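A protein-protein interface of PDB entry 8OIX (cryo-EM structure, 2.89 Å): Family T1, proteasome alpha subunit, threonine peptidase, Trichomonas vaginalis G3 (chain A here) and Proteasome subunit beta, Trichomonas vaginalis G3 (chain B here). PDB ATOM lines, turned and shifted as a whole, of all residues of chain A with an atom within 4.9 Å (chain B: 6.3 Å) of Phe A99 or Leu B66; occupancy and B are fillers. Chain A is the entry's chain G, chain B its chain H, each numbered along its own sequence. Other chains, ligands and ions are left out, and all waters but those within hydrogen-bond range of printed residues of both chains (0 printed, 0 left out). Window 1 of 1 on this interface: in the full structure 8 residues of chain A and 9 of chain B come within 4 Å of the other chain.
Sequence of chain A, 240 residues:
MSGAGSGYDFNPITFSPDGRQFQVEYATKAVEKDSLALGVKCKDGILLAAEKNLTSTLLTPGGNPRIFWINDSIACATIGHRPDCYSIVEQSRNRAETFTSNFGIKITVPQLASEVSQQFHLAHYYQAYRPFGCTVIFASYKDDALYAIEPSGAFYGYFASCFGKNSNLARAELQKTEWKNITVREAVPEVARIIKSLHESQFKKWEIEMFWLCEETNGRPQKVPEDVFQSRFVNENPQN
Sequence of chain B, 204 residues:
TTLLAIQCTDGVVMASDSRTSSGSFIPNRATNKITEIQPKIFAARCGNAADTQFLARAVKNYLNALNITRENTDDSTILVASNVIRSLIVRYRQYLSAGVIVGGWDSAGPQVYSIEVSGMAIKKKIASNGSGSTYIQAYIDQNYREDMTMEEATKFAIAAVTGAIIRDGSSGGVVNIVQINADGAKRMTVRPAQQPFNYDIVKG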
ATOM      1  N   ASN A  94      -6.877 -11.491   1.453  1.00  0.00           N
ATOM      2  CA  ASN A  94      -7.928 -12.043   0.604  1.00  0.00           C
ATOM      3  C   ASN A  94      -7.468 -12.159  -0.843  1.00  0.00           C
ATOM      4  O   ASN A  94      -7.814 -13.123  -1.532  1.00  0.00           O
ATOM      5  CB  ASN A  94      -9.186 -11.182   0.697  1.00  0.00           C
ATOM      6  CG  ASN A  94      -9.941 -11.394   1.991  1.00  0.00           C
ATOM      7  OD1 ASN A  94      -9.617 -12.288   2.773  1.00  0.00           O
ATOM      8  ND2 ASN A  94     -10.956 -10.572   2.224  1.00  0.00           N
ATOM      9  N   ARG A  95      -6.700 -11.180  -1.328  1.00  0.00           N
ATOM     10  CA  ARG A  95      -6.191 -11.236  -2.693  1.00  0.00           C
ATOM     11  C   ARG A  95      -5.198 -12.375  -2.859  1.00  0.00           C
ATOM     12  O   ARG A  95      -5.203 -13.061  -3.883  1.00  0.00           O
ATOM     13  CB  ARG A  95      -5.543  -9.904  -3.069  1.00  0.00           C
ATOM     14  CG  ARG A  95      -6.524  -8.836  -3.518  1.00  0.00           C
ATOM     15  CD  ARG A  95      -7.118  -9.167  -4.874  1.00  0.00           C
ATOM     16  NE  ARG A  95      -7.951  -8.085  -5.382  1.00  0.00           N
ATOM     17  CZ  ARG A  95      -8.323  -7.955  -6.648  1.00  0.00           C
ATOM     18  NH1 ARG A  95      -7.942  -8.822  -7.573  1.00  0.00           N
ATOM     19  NH2 ARG A  95      -9.094  -6.930  -6.997  1.00  0.00           N
ATOM     20  N   ALA A  96      -4.343 -12.596  -1.859  1.00  0.00           N
ATOM     21  CA  ALA A  96      -3.427 -13.729  -1.903  1.00  0.00           C
ATOM     22  C   ALA A  96      -4.181 -15.052  -1.873  1.00  0.00           C
ATOM     23  O   ALA A  96      -3.838 -15.987  -2.605  1.00  0.00           O
ATOM     24  CB  ALA A  96      -2.435 -13.646  -0.744  1.00  0.00           C
ATOM     25  N   GLU A  97      -5.208 -15.155  -1.025  1.00  0.00           N
ATOM     26  CA  GLU A  97      -6.003 -16.378  -0.974  1.00  0.00           C
ATOM     27  C   GLU A  97      -6.725 -16.625  -2.292  1.00  0.00           C
ATOM     28  O   GLU A  97      -6.777 -17.761  -2.777  1.00  0.00           O
ATOM     29  CB  GLU A  97      -7.001 -16.317   0.182  1.00  0.00           C
ATOM     30  CG  GLU A  97      -6.367 -16.321   1.570  1.00  0.00           C
ATOM     31  CD  GLU A  97      -5.642 -17.615   1.906  1.00  0.00           C
ATOM     32  OE1 GLU A  97      -5.765 -18.601   1.147  1.00  0.00           O
ATOM     33  OE2 GLU A  97      -4.938 -17.644   2.936  1.00  0.00           O
ATOM     34  N   THR A  98      -7.299 -15.575  -2.883  1.00  0.00           N
ATOM     35  CA  THR A  98      -7.973 -15.716  -4.170  1.00  0.00           C
ATOM     36  C   THR A  98      -6.982 -16.072  -5.266  1.00  0.00           C
ATOM     37  O   THR A  98      -7.299 -16.848  -6.174  1.00  0.00           O
ATOM     38  CB  THR A  98      -8.714 -14.426  -4.516  1.00  0.00           C
ATOM     39  OG1 THR A  98      -9.452 -13.975  -3.375  1.00  0.00           O
ATOM     40  CG2 THR A  98      -9.673 -14.657  -5.669  1.00  0.00           C
ATOM     41  N   PHE A  99      -5.777 -15.505  -5.201  1.00  0.00           N
ATOM     42  CA  PHE A  99      -4.732 -15.838  -6.156  1.00  0.00           C
ATOM     43  C   PHE A  99      -4.337 -17.302  -6.042  1.00  0.00           C
ATOM     44  O   PHE A  99      -4.113 -17.972  -7.055  1.00  0.00           O
ATOM     45  CB  PHE A  99      -3.526 -14.929  -5.923  1.00  0.00           C
ATOM     46  CG  PHE A  99      -2.369 -15.213  -6.824  1.00  0.00           C
ATOM     47  CD1 PHE A  99      -2.254 -14.568  -8.038  1.00  0.00           C
ATOM     48  CD2 PHE A  99      -1.394 -16.123  -6.459  1.00  0.00           C
ATOM     49  CE1 PHE A  99      -1.194 -14.827  -8.868  1.00  0.00           C
ATOM     50  CE2 PHE A  99      -0.333 -16.384  -7.286  1.00  0.00           C
ATOM     51  CZ  PHE A  99      -0.230 -15.736  -8.491  1.00  0.00           C
ATOM     52  N   THR A 100      -4.225 -17.811  -4.815  1.00  0.00           N
ATOM     53  CA  THR A 100      -3.939 -19.230  -4.627  1.00  0.00           C
ATOM     54  C   THR A 100      -5.086 -20.093  -5.139  1.00  0.00           C
ATOM     55  O   THR A 100      -4.860 -21.130  -5.772  1.00  0.00           O
ATOM     56  CB  THR A 100      -3.660 -19.516  -3.152  1.00  0.00           C
ATOM     57  OG1 THR A 100      -2.414 -18.918  -2.778  1.00  0.00           O
ATOM     58  CG2 THR A 100      -3.586 -21.012  -2.897  1.00  0.00           C
ATOM     59  N   SER A 101      -6.327 -19.676  -4.882  1.00  0.00           N
ATOM     60  CA  SER A 101      -7.474 -20.441  -5.356  1.00  0.00           C
ATOM     61  C   SER A 101      -7.503 -20.507  -6.877  1.00  0.00           C
ATOM     62  O   SER A 101      -7.772 -21.565  -7.457  1.00  0.00           O
ATOM     63  CB  SER A 101      -8.767 -19.825  -4.823  1.00  0.00           C
ATOM     64  OG  SER A 101      -8.705 -19.648  -3.421  1.00  0.00           O
ATOM     65  N   ASN A 102      -7.227 -19.383  -7.539  1.00  0.00           N
ATOM     66  CA  ASN A 102      -7.282 -19.330  -8.994  1.00  0.00           C
ATOM     67  C   ASN A 102      -6.067 -19.973  -9.650  1.00  0.00           C
ATOM     68  O   ASN A 102      -6.193 -20.552 -10.733  1.00  0.00           O
ATOM     69  CB  ASN A 102      -7.414 -17.879  -9.459  1.00  0.00           C
ATOM     70  CG  ASN A 102      -8.680 -17.219  -8.956  1.00  0.00           C
ATOM     71  OD1 ASN A 102      -9.669 -17.889  -8.663  1.00  0.00           O
ATOM     72  ND2 ASN A 102      -8.656 -15.895  -8.853  1.00  0.00           N
ATOM     73  N   PHE A 103      -4.895 -19.892  -9.017  1.00  0.00           N
ATOM     74  CA  PHE A 103      -3.645 -20.282  -9.651  1.00  0.00           C
ATOM     75  C   PHE A 103      -2.815 -21.291  -8.866  1.00  0.00           C
ATOM     76  O   PHE A 103      -1.818 -21.783  -9.407  1.00  0.00           O
ATOM     77  CB  PHE A 103      -2.783 -19.040  -9.919  1.00  0.00           C
ATOM     78  CG  PHE A 103      -3.513 -17.947 -10.645  1.00  0.00           C
ATOM     79  CD1 PHE A 103      -3.845 -18.083 -11.980  1.00  0.00           C
ATOM     80  CD2 PHE A 103      -3.874 -16.786  -9.988  1.00  0.00           C
ATOM     81  CE1 PHE A 103      -4.516 -17.080 -12.648  1.00  0.00           C
ATOM     82  CE2 PHE A 103      -4.544 -15.778 -10.651  1.00  0.00           C
ATOM     83  CZ  PHE A 103      -4.867 -15.926 -11.982  1.00  0.00           C
ATOM     84  N   GLY A 104      -3.177 -21.612  -7.628  1.00  0.00           N
ATOM     85  CA  GLY A 104      -2.493 -22.654  -6.885  1.00  0.00           C
ATOM     86  C   GLY A 104      -1.210 -22.242  -6.190  1.00  0.00           C
ATOM     87  O   GLY A 104      -0.935 -22.704  -5.081  1.00  0.00           O
ATOM     88  N   ILE A 105      -0.414 -21.380  -6.819  1.00  0.00           N
ATOM     89  CA  ILE A 105       0.841 -20.933  -6.224  1.00  0.00           C
ATOM     90  C   ILE A 105       0.563 -19.806  -5.241  1.00  0.00           C
ATOM     91  O   ILE A 105      -0.559 -19.291  -5.168  1.00  0.00           O
ATOM     92  CB  ILE A 105       1.853 -20.478  -7.290  1.00  0.00           C
ATOM     93  CG1 ILE A 105       1.292 -19.310  -8.097  1.00  0.00           C
ATOM     94  CG2 ILE A 105       2.205 -21.627  -8.211  1.00  0.00           C
ATOM     95  CD1 ILE A 105       2.330 -18.597  -8.931  1.00  0.00           C
ATOM     96  N   LYS A 106       1.578 -19.420  -4.475  1.00  0.00           N
ATOM     97  CA  LYS A 106       1.469 -18.292  -3.563  1.00  0.00           C
ATOM     98  C   LYS A 106       1.840 -17.011  -4.295  1.00  0.00           C
ATOM     99  O   LYS A 106       2.747 -16.997  -5.132  1.00  0.00           O
ATOM    100  CB  LYS A 106       2.372 -18.485  -2.345  1.00  0.00           C
ATOM    101  CG  LYS A 106       1.998 -19.677  -1.484  1.00  0.00           C
ATOM    102  CD  LYS A 106       0.571 -19.559  -0.980  1.00  0.00           C
ATOM    103  CE  LYS A 106       0.211 -20.716  -0.065  1.00  0.00           C
ATOM    104  NZ  LYS A 106       0.373 -22.032  -0.741  1.00  0.00           N
ATOM    105  N   ILE A 107       1.121 -15.933  -3.977  1.00  0.00           N
ATOM    106  CA  ILE A 107       1.279 -14.687  -4.715  1.00  0.00           C
ATOM    107  C   ILE A 107       2.659 -14.086  -4.455  1.00  0.00           C
ATOM    108  O   ILE A 107       3.320 -14.367  -3.448  1.00  0.00           O
ATOM    109  CB  ILE A 107       0.152 -13.710  -4.343  1.00  0.00           C
ATOM    110  CG1 ILE A 107       0.011 -12.604  -5.388  1.00  0.00           C
ATOM    111  CG2 ILE A 107       0.396 -13.110  -2.973  1.00  0.00           C
ATOM    112  CD1 ILE A 107      -1.308 -11.880  -5.316  1.00  0.00           C
ATOM    113  N   GLN A 111       2.990  -8.645  -7.964  1.00  0.00           N
ATOM    114  CA  GLN A 111       1.616  -8.768  -8.428  1.00  0.00           C
ATOM    115  C   GLN A 111       0.606  -8.655  -7.295  1.00  0.00           C
ATOM    116  O   GLN A 111      -0.527  -8.227  -7.533  1.00  0.00           O
ATOM    117  CB  GLN A 111       1.437 -10.072  -9.201  1.00  0.00           C
ATOM    118  CG  GLN A 111       1.441 -11.328  -8.378  1.00  0.00           C
ATOM    119  CD  GLN A 111       1.241 -12.553  -9.238  1.00  0.00           C
ATOM    120  OE1 GLN A 111       0.391 -12.562 -10.129  1.00  0.00           O
ATOM    121  NE2 GLN A 111       2.030 -13.590  -8.989  1.00  0.00           N
ATOM    122  N   GLU A 115      -2.420  -6.052  -7.492  1.00  0.00           N
ATOM    123  CA  GLU A 115      -3.803  -6.400  -7.180  1.00  0.00           C
ATOM    124  C   GLU A 115      -4.380  -5.521  -6.077  1.00  0.00           C
ATOM    125  O   GLU A 115      -5.576  -5.214  -6.096  1.00  0.00           O
ATOM    126  CB  GLU A 115      -3.896  -7.873  -6.784  1.00  0.00           C
ATOM    127  CG  GLU A 115      -3.606  -8.840  -7.917  1.00  0.00           C
ATOM    128  CD  GLU A 115      -4.172 -10.223  -7.662  1.00  0.00           C
ATOM    129  OE1 GLU A 115      -4.507 -10.524  -6.499  1.00  0.00           O
ATOM    130  OE2 GLU A 115      -4.281 -11.007  -8.628  1.00  0.00           O
ATOM    131  N   ASN B  61      -6.583 -18.458 -21.100  1.00  0.00           N
ATOM    132  CA  ASN B  61      -7.199 -17.301 -20.459  1.00  0.00           C
ATOM    133  C   ASN B  61      -6.707 -17.128 -19.025  1.00  0.00           C
ATOM    134  O   ASN B  61      -6.419 -16.009 -18.593  1.00  0.00           O
ATOM    135  CB  ASN B  61      -8.720 -17.438 -20.488  1.00  0.00           C
ATOM    136  CG  ASN B  61      -9.426 -16.205 -19.965  1.00  0.00           C
ATOM    137  OD1 ASN B  61      -8.864 -15.111 -19.954  1.00  0.00           O
ATOM    138  ND2 ASN B  61     -10.665 -16.378 -19.526  1.00  0.00           N
ATOM    139  N   TYR B  62      -6.603 -18.227 -18.276  1.00  0.00           N
ATOM    140  CA  TYR B  62      -6.192 -18.157 -16.876  1.00  0.00           C
ATOM    141  C   TYR B  62      -4.732 -17.750 -16.738  1.00  0.00           C
ATOM    142  O   TYR B  62      -4.371 -17.035 -15.799  1.00  0.00           O
ATOM    143  CB  TYR B  62      -6.436 -19.501 -16.191  1.00  0.00           C
ATOM    144  CG  TYR B  62      -7.765 -19.616 -15.480  1.00  0.00           C
ATOM    145  CD1 TYR B  62      -8.951 -19.728 -16.192  1.00  0.00           C
ATOM    146  CD2 TYR B  62      -7.833 -19.626 -14.093  1.00  0.00           C
ATOM    147  CE1 TYR B  62     -10.167 -19.838 -15.544  1.00  0.00           C
ATOM    148  CE2 TYR B  62      -9.042 -19.739 -13.436  1.00  0.00           C
ATOM    149  CZ  TYR B  62     -10.207 -19.843 -14.165  1.00  0.00           C
ATOM    150  OH  TYR B  62     -11.414 -19.953 -13.513  1.00  0.00           O
ATOM    151  N   LEU B  63      -3.874 -18.203 -17.652  1.00  0.00           N
ATOM    152  CA  LEU B  63      -2.467 -17.828 -17.597  1.00  0.00           C
ATOM    153  C   LEU B  63      -2.246 -16.400 -18.063  1.00  0.00           C
ATOM    154  O   LEU B  63      -1.335 -15.728 -17.570  1.00  0.00           O
ATOM    155  CB  LEU B  63      -1.623 -18.789 -18.435  1.00  0.00           C
ATOM    156  CG  LEU B  63      -1.488 -20.214 -17.901  1.00  0.00           C
ATOM    157  CD1 LEU B  63      -0.580 -21.028 -18.795  1.00  0.00           C
ATOM    158  CD2 LEU B  63      -0.955 -20.194 -16.486  1.00  0.00           C
ATOM    159  N   ASN B  64      -3.053 -15.923 -19.013  1.00  0.00           N
ATOM    160  CA  ASN B  64      -3.022 -14.501 -19.334  1.00  0.00           C
ATOM    161  C   ASN B  64      -3.540 -13.668 -18.169  1.00  0.00           C
ATOM    162  O   ASN B  64      -3.034 -12.570 -17.910  1.00  0.00           O
ATOM    163  CB  ASN B  64      -3.829 -14.234 -20.602  1.00  0.00           C
ATOM    164  CG  ASN B  64      -3.289 -14.973 -21.807  1.00  0.00           C
ATOM    165  OD1 ASN B  64      -2.117 -15.341 -21.851  1.00  0.00           O
ATOM    166  ND2 ASN B  64      -4.144 -15.187 -22.800  1.00  0.00           N
ATOM    167  N   ALA B  65      -4.554 -14.172 -17.459  1.00  0.00           N
ATOM    168  CA  ALA B  65      -5.039 -13.503 -16.257  1.00  0.00           C
ATOM    169  C   ALA B  65      -3.958 -13.453 -15.188  1.00  0.00           C
ATOM    170  O   ALA B  65      -3.828 -12.456 -14.468  1.00  0.00           O
ATOM    171  CB  ALA B  65      -6.287 -14.209 -15.729  1.00  0.00           C
ATOM    172  N   LEU B  66      -3.188 -14.533 -15.058  1.00  0.00           N
ATOM    173  CA  LEU B  66      -2.044 -14.547 -14.157  1.00  0.00           C
ATOM    174  C   LEU B  66      -1.065 -13.431 -14.490  1.00  0.00           C
ATOM    175  O   LEU B  66      -0.368 -12.928 -13.603  1.00  0.00           O
ATOM    176  CB  LEU B  66      -1.352 -15.907 -14.237  1.00  0.00           C
ATOM    177  CG  LEU B  66      -0.075 -16.148 -13.436  1.00  0.00           C
ATOM    178  CD1 LEU B  66      -0.365 -16.137 -11.956  1.00  0.00           C
ATOM    179  CD2 LEU B  66       0.559 -17.461 -13.850  1.00  0.00           C
ATOM    180  N   ASN B  67      -1.012 -13.026 -15.754  1.00  0.00           N
ATOM    181  CA  ASN B  67      -0.092 -12.005 -16.227  1.00  0.00           C
ATOM    182  C   ASN B  67      -0.688 -10.603 -16.202  1.00  0.00           C
ATOM    183  O   ASN B  67       0.017  -9.645 -16.533  1.00  0.00           O
ATOM    184  CB  ASN B  67       0.372 -12.344 -17.645  1.00  0.00           C
ATOM    185  CG  ASN B  67       1.015 -13.712 -17.733  1.00  0.00           C
ATOM    186  OD1 ASN B  67       1.620 -14.188 -16.773  1.00  0.00           O
ATOM    187  ND2 ASN B  67       0.886 -14.354 -18.886  1.00  0.00           N
ATOM    188  N   ILE B  68      -1.964 -10.461 -15.832  1.00  0.00           N
ATOM    189  CA  ILE B  68      -2.577  -9.135 -15.774  1.00  0.00           C
ATOM    190  C   ILE B  68      -1.851  -8.251 -14.770  1.00  0.00           C
ATOM    191  O   ILE B  68      -1.628  -7.059 -15.015  1.00  0.00           O
ATOM    192  CB  ILE B  68      -4.075  -9.241 -15.437  1.00  0.00           C
ATOM    193  CG1 ILE B  68      -4.847  -9.906 -16.567  1.00  0.00           C
ATOM    194  CG2 ILE B  68      -4.660  -7.878 -15.168  1.00  0.00           C
ATOM    195  CD1 ILE B  68      -6.295 -10.180 -16.224  1.00  0.00           C
ATOM    196  N   THR B  69      -1.466  -8.817 -13.630  1.00  0.00           N
ATOM    197  CA  THR B  69      -0.927  -8.033 -12.529  1.00  0.00           C
ATOM    198  C   THR B  69       0.548  -8.309 -12.275  1.00  0.00           C
ATOM    199  O   THR B  69       1.109  -7.768 -11.319  1.00  0.00           O
ATOM    200  CB  THR B  69      -1.735  -8.295 -11.257  1.00  0.00           C
ATOM    201  OG1 THR B  69      -1.832  -9.707 -11.034  1.00  0.00           O
ATOM    202  CG2 THR B  69      -3.133  -7.717 -11.389  1.00  0.00           C
ATOM    203  N   ARG B  70       1.203  -9.094 -13.126  1.00  0.00           N
ATOM    204  CA  ARG B  70       2.600  -9.441 -12.922  1.00  0.00           C
ATOM    205  C   ARG B  70       3.382  -9.249 -14.212  1.00  0.00           C
ATOM    206  O   ARG B  70       2.828  -9.257 -15.314  1.00  0.00           O
ATOM    207  CB  ARG B  70       2.762 -10.887 -12.435  1.00  0.00           C
ATOM    208  CG  ARG B  70       2.753 -11.917 -13.547  1.00  0.00           C
ATOM    209  CD  ARG B  70       2.914 -13.323 -13.007  1.00  0.00           C
ATOM    210  NE  ARG B  70       3.024 -14.297 -14.086  1.00  0.00           N
ATOM    211  CZ  ARG B  70       3.416 -15.553 -13.924  1.00  0.00           C
ATOM    212  NH1 ARG B  70       3.744 -16.027 -12.735  1.00  0.00           N
ATOM    213  NH2 ARG B  70       3.487 -16.351 -14.985  1.00  0.00           N
ATOM    214  N   THR B  73       6.145 -13.098 -16.413  1.00  0.00           N
ATOM    215  CA  THR B  73       5.157 -13.936 -17.085  1.00  0.00           C
ATOM    216  C   THR B  73       5.625 -15.375 -17.264  1.00  0.00           C
ATOM    217  O   THR B  73       4.786 -16.272 -17.402  1.00  0.00           O
ATOM    218  CB  THR B  73       4.808 -13.335 -18.445  1.00  0.00           C
ATOM    219  OG1 THR B  73       6.014 -13.052 -19.164  1.00  0.00           O
ATOM    220  CG2 THR B  73       4.029 -12.049 -18.263  1.00  0.00           C
ATOM    221  N   ASP B  75       7.148 -17.277 -15.020  1.00  0.00           N
ATOM    222  CA  ASP B  75       7.477 -17.733 -13.676  1.00  0.00           C
ATOM    223  C   ASP B  75       6.304 -18.537 -13.134  1.00  0.00           C
ATOM    224  O   ASP B  75       5.175 -18.039 -13.092  1.00  0.00           O
ATOM    225  CB  ASP B  75       7.797 -16.544 -12.763  1.00  0.00           C
ATOM    226  CG  ASP B  75       8.356 -16.966 -11.413  1.00  0.00           C
ATOM    227  OD1 ASP B  75       7.729 -17.799 -10.725  1.00  0.00           O
ATOM    228  OD2 ASP B  75       9.432 -16.457 -11.038  1.00  0.00           O
ATOM    229  N   SER B  76       6.577 -19.779 -12.727  1.00  0.00           N
ATOM    230  CA  SER B  76       5.577 -20.698 -12.181  1.00  0.00           C
ATOM    231  C   SER B  76       4.410 -20.922 -13.133  1.00  0.00           C
ATOM    232  O   SER B  76       3.326 -21.326 -12.705  1.00  0.00           O
ATOM    233  CB  SER B  76       5.058 -20.215 -10.821  1.00  0.00           C
ATOM    234  OG  SER B  76       6.070 -20.280  -9.833  1.00  0.00           O
ATOM    235  N   THR B  77       4.616 -20.672 -14.427  1.00  0.00           N
ATOM    236  CA  THR B  77       3.511 -20.714 -15.377  1.00  0.00           C
ATOM    237  C   THR B  77       3.020 -22.139 -15.602  1.00  0.00           C
ATOM    238  O   THR B  77       1.818 -22.364 -15.766  1.00  0.00           O
ATOM    239  CB  THR B  77       3.933 -20.069 -16.697  1.00  0.00           C
ATOM    240  OG1 THR B  77       4.245 -18.689 -16.472  1.00  0.00           O
ATOM    241  CG2 THR B  77       2.812 -20.149 -17.710  1.00  0.00           C
ATOM    242  N   VAL B  80       1.063 -23.191 -12.475  1.00  0.00           N
ATOM    243  CA  VAL B  80      -0.232 -22.517 -12.476  1.00  0.00           C
ATOM    244  C   VAL B  80      -1.139 -23.106 -13.547  1.00  0.00           C
ATOM    245  O   VAL B  80      -2.352 -23.223 -13.352  1.00  0.00           O
ATOM    246  CB  VAL B  80      -0.049 -21.002 -12.660  1.00  0.00           C
ATOM    247  CG1 VAL B  80      -1.380 -20.340 -12.942  1.00  0.00           C
ATOM    248  CG2 VAL B  80       0.574 -20.402 -11.429  1.00  0.00           C
ATOM    249  N   ALA B  81      -0.573 -23.481 -14.694  1.00  0.00           N
ATOM    250  CA  ALA B  81      -1.366 -24.112 -15.742  1.00  0.00           C
ATOM    251  C   ALA B  81      -1.939 -25.435 -15.260  1.00  0.00           C
ATOM    252  O   ALA B  81      -3.114 -25.737 -15.482  1.00  0.00           O
ATOM    253  CB  ALA B  81      -0.516 -24.313 -16.996  1.00  0.00           C
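The guanidinium group (NH1) of Arg A95 lies within salt-bridge range of the side-chain carboxylate (OE1) of Glu A115 (3.98 Å). The side-chain hydroxyl (OG1) of Thr A100 sits at hydrogen-bond distance from the backbone carbonyl oxygen (O) of Ile A105, 3.0 Å away. OD1 of Asn B67 sits at hydrogen-bond distance from NE of Arg B70 (3.0 Å). The backbone carbonyl oxygen of Asp B75 is in hydrogen-bond range of the guanidinium group of Arg B70. The side-chain hydroxyl (OG1) of Thr B77 lies within hydrogen-bond range of the guanidinium group (NH2) of Arg B70 (2.9 Å). OG of Ser B76 is in hydrogen-bond range of OD1 of Asp B75 (3.1 Å).
Phe A99 touches Leu B66. O of Asn A102 touches CD2 of Tyr B62, at 3.9 Å. Tyr B62 touches Phe A103 (O to CE1, 3.2 Å). CB of Leu B66 touches CE1 of Phe A103, 3.7 Å away. Val B80 touches Phe A103. Ile A105 touches Ser B76. CG2 of Val B80 touches CD1 of Ile A105, at 3.5 Å. Gln A111 touches Leu B66. Gln A111 touches Arg B70. Glu A115 touches Thr B69.
Phe A99 touches just one residue of chain B: Leu B66 (3.5 Å). Leu B66 touches just these residues of chain A: Phe A99 (3.5 Å), Phe A103 (3.7 Å) and Gln A111 (3.6 Å). Of the printed residues of chain A, Arg B70 touches Gln A111. Of the printed residues of chain B, Phe A103 touches Tyr B62, Leu B66 and Val B80. Printed residues of chain B within 4 Å of Glu A115: Thr B69. The nearest printed residue of chain B that does not touch Phe A99 is Val B80 (5.6 Å).
Of the 16 printed residues of chain B, 6 touch a printed residue of chain A. Printed residues of chain B that touch a printed residue of chain A: Tyr B62, Leu B66, Thr B69, Arg B70, Ser B76 and Val B80. Hydrophobic or aromatic side chains of chain B that line the printed part of chain A: Tyr B62, Leu B66 and Val B80. Of the 16 printed residues of chain A, 6 touch a printed residue of chain B. Printed residues of chain A that touch a printed residue of chain B: Phe A99, Asn A102, Phe A103, Ile A105, Gln A111 and Glu A115. Among the printed residues, no Asp or Glu carboxylate lies within 4 Å of a Lys or Arg side-chain nitrogen of the other chain.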
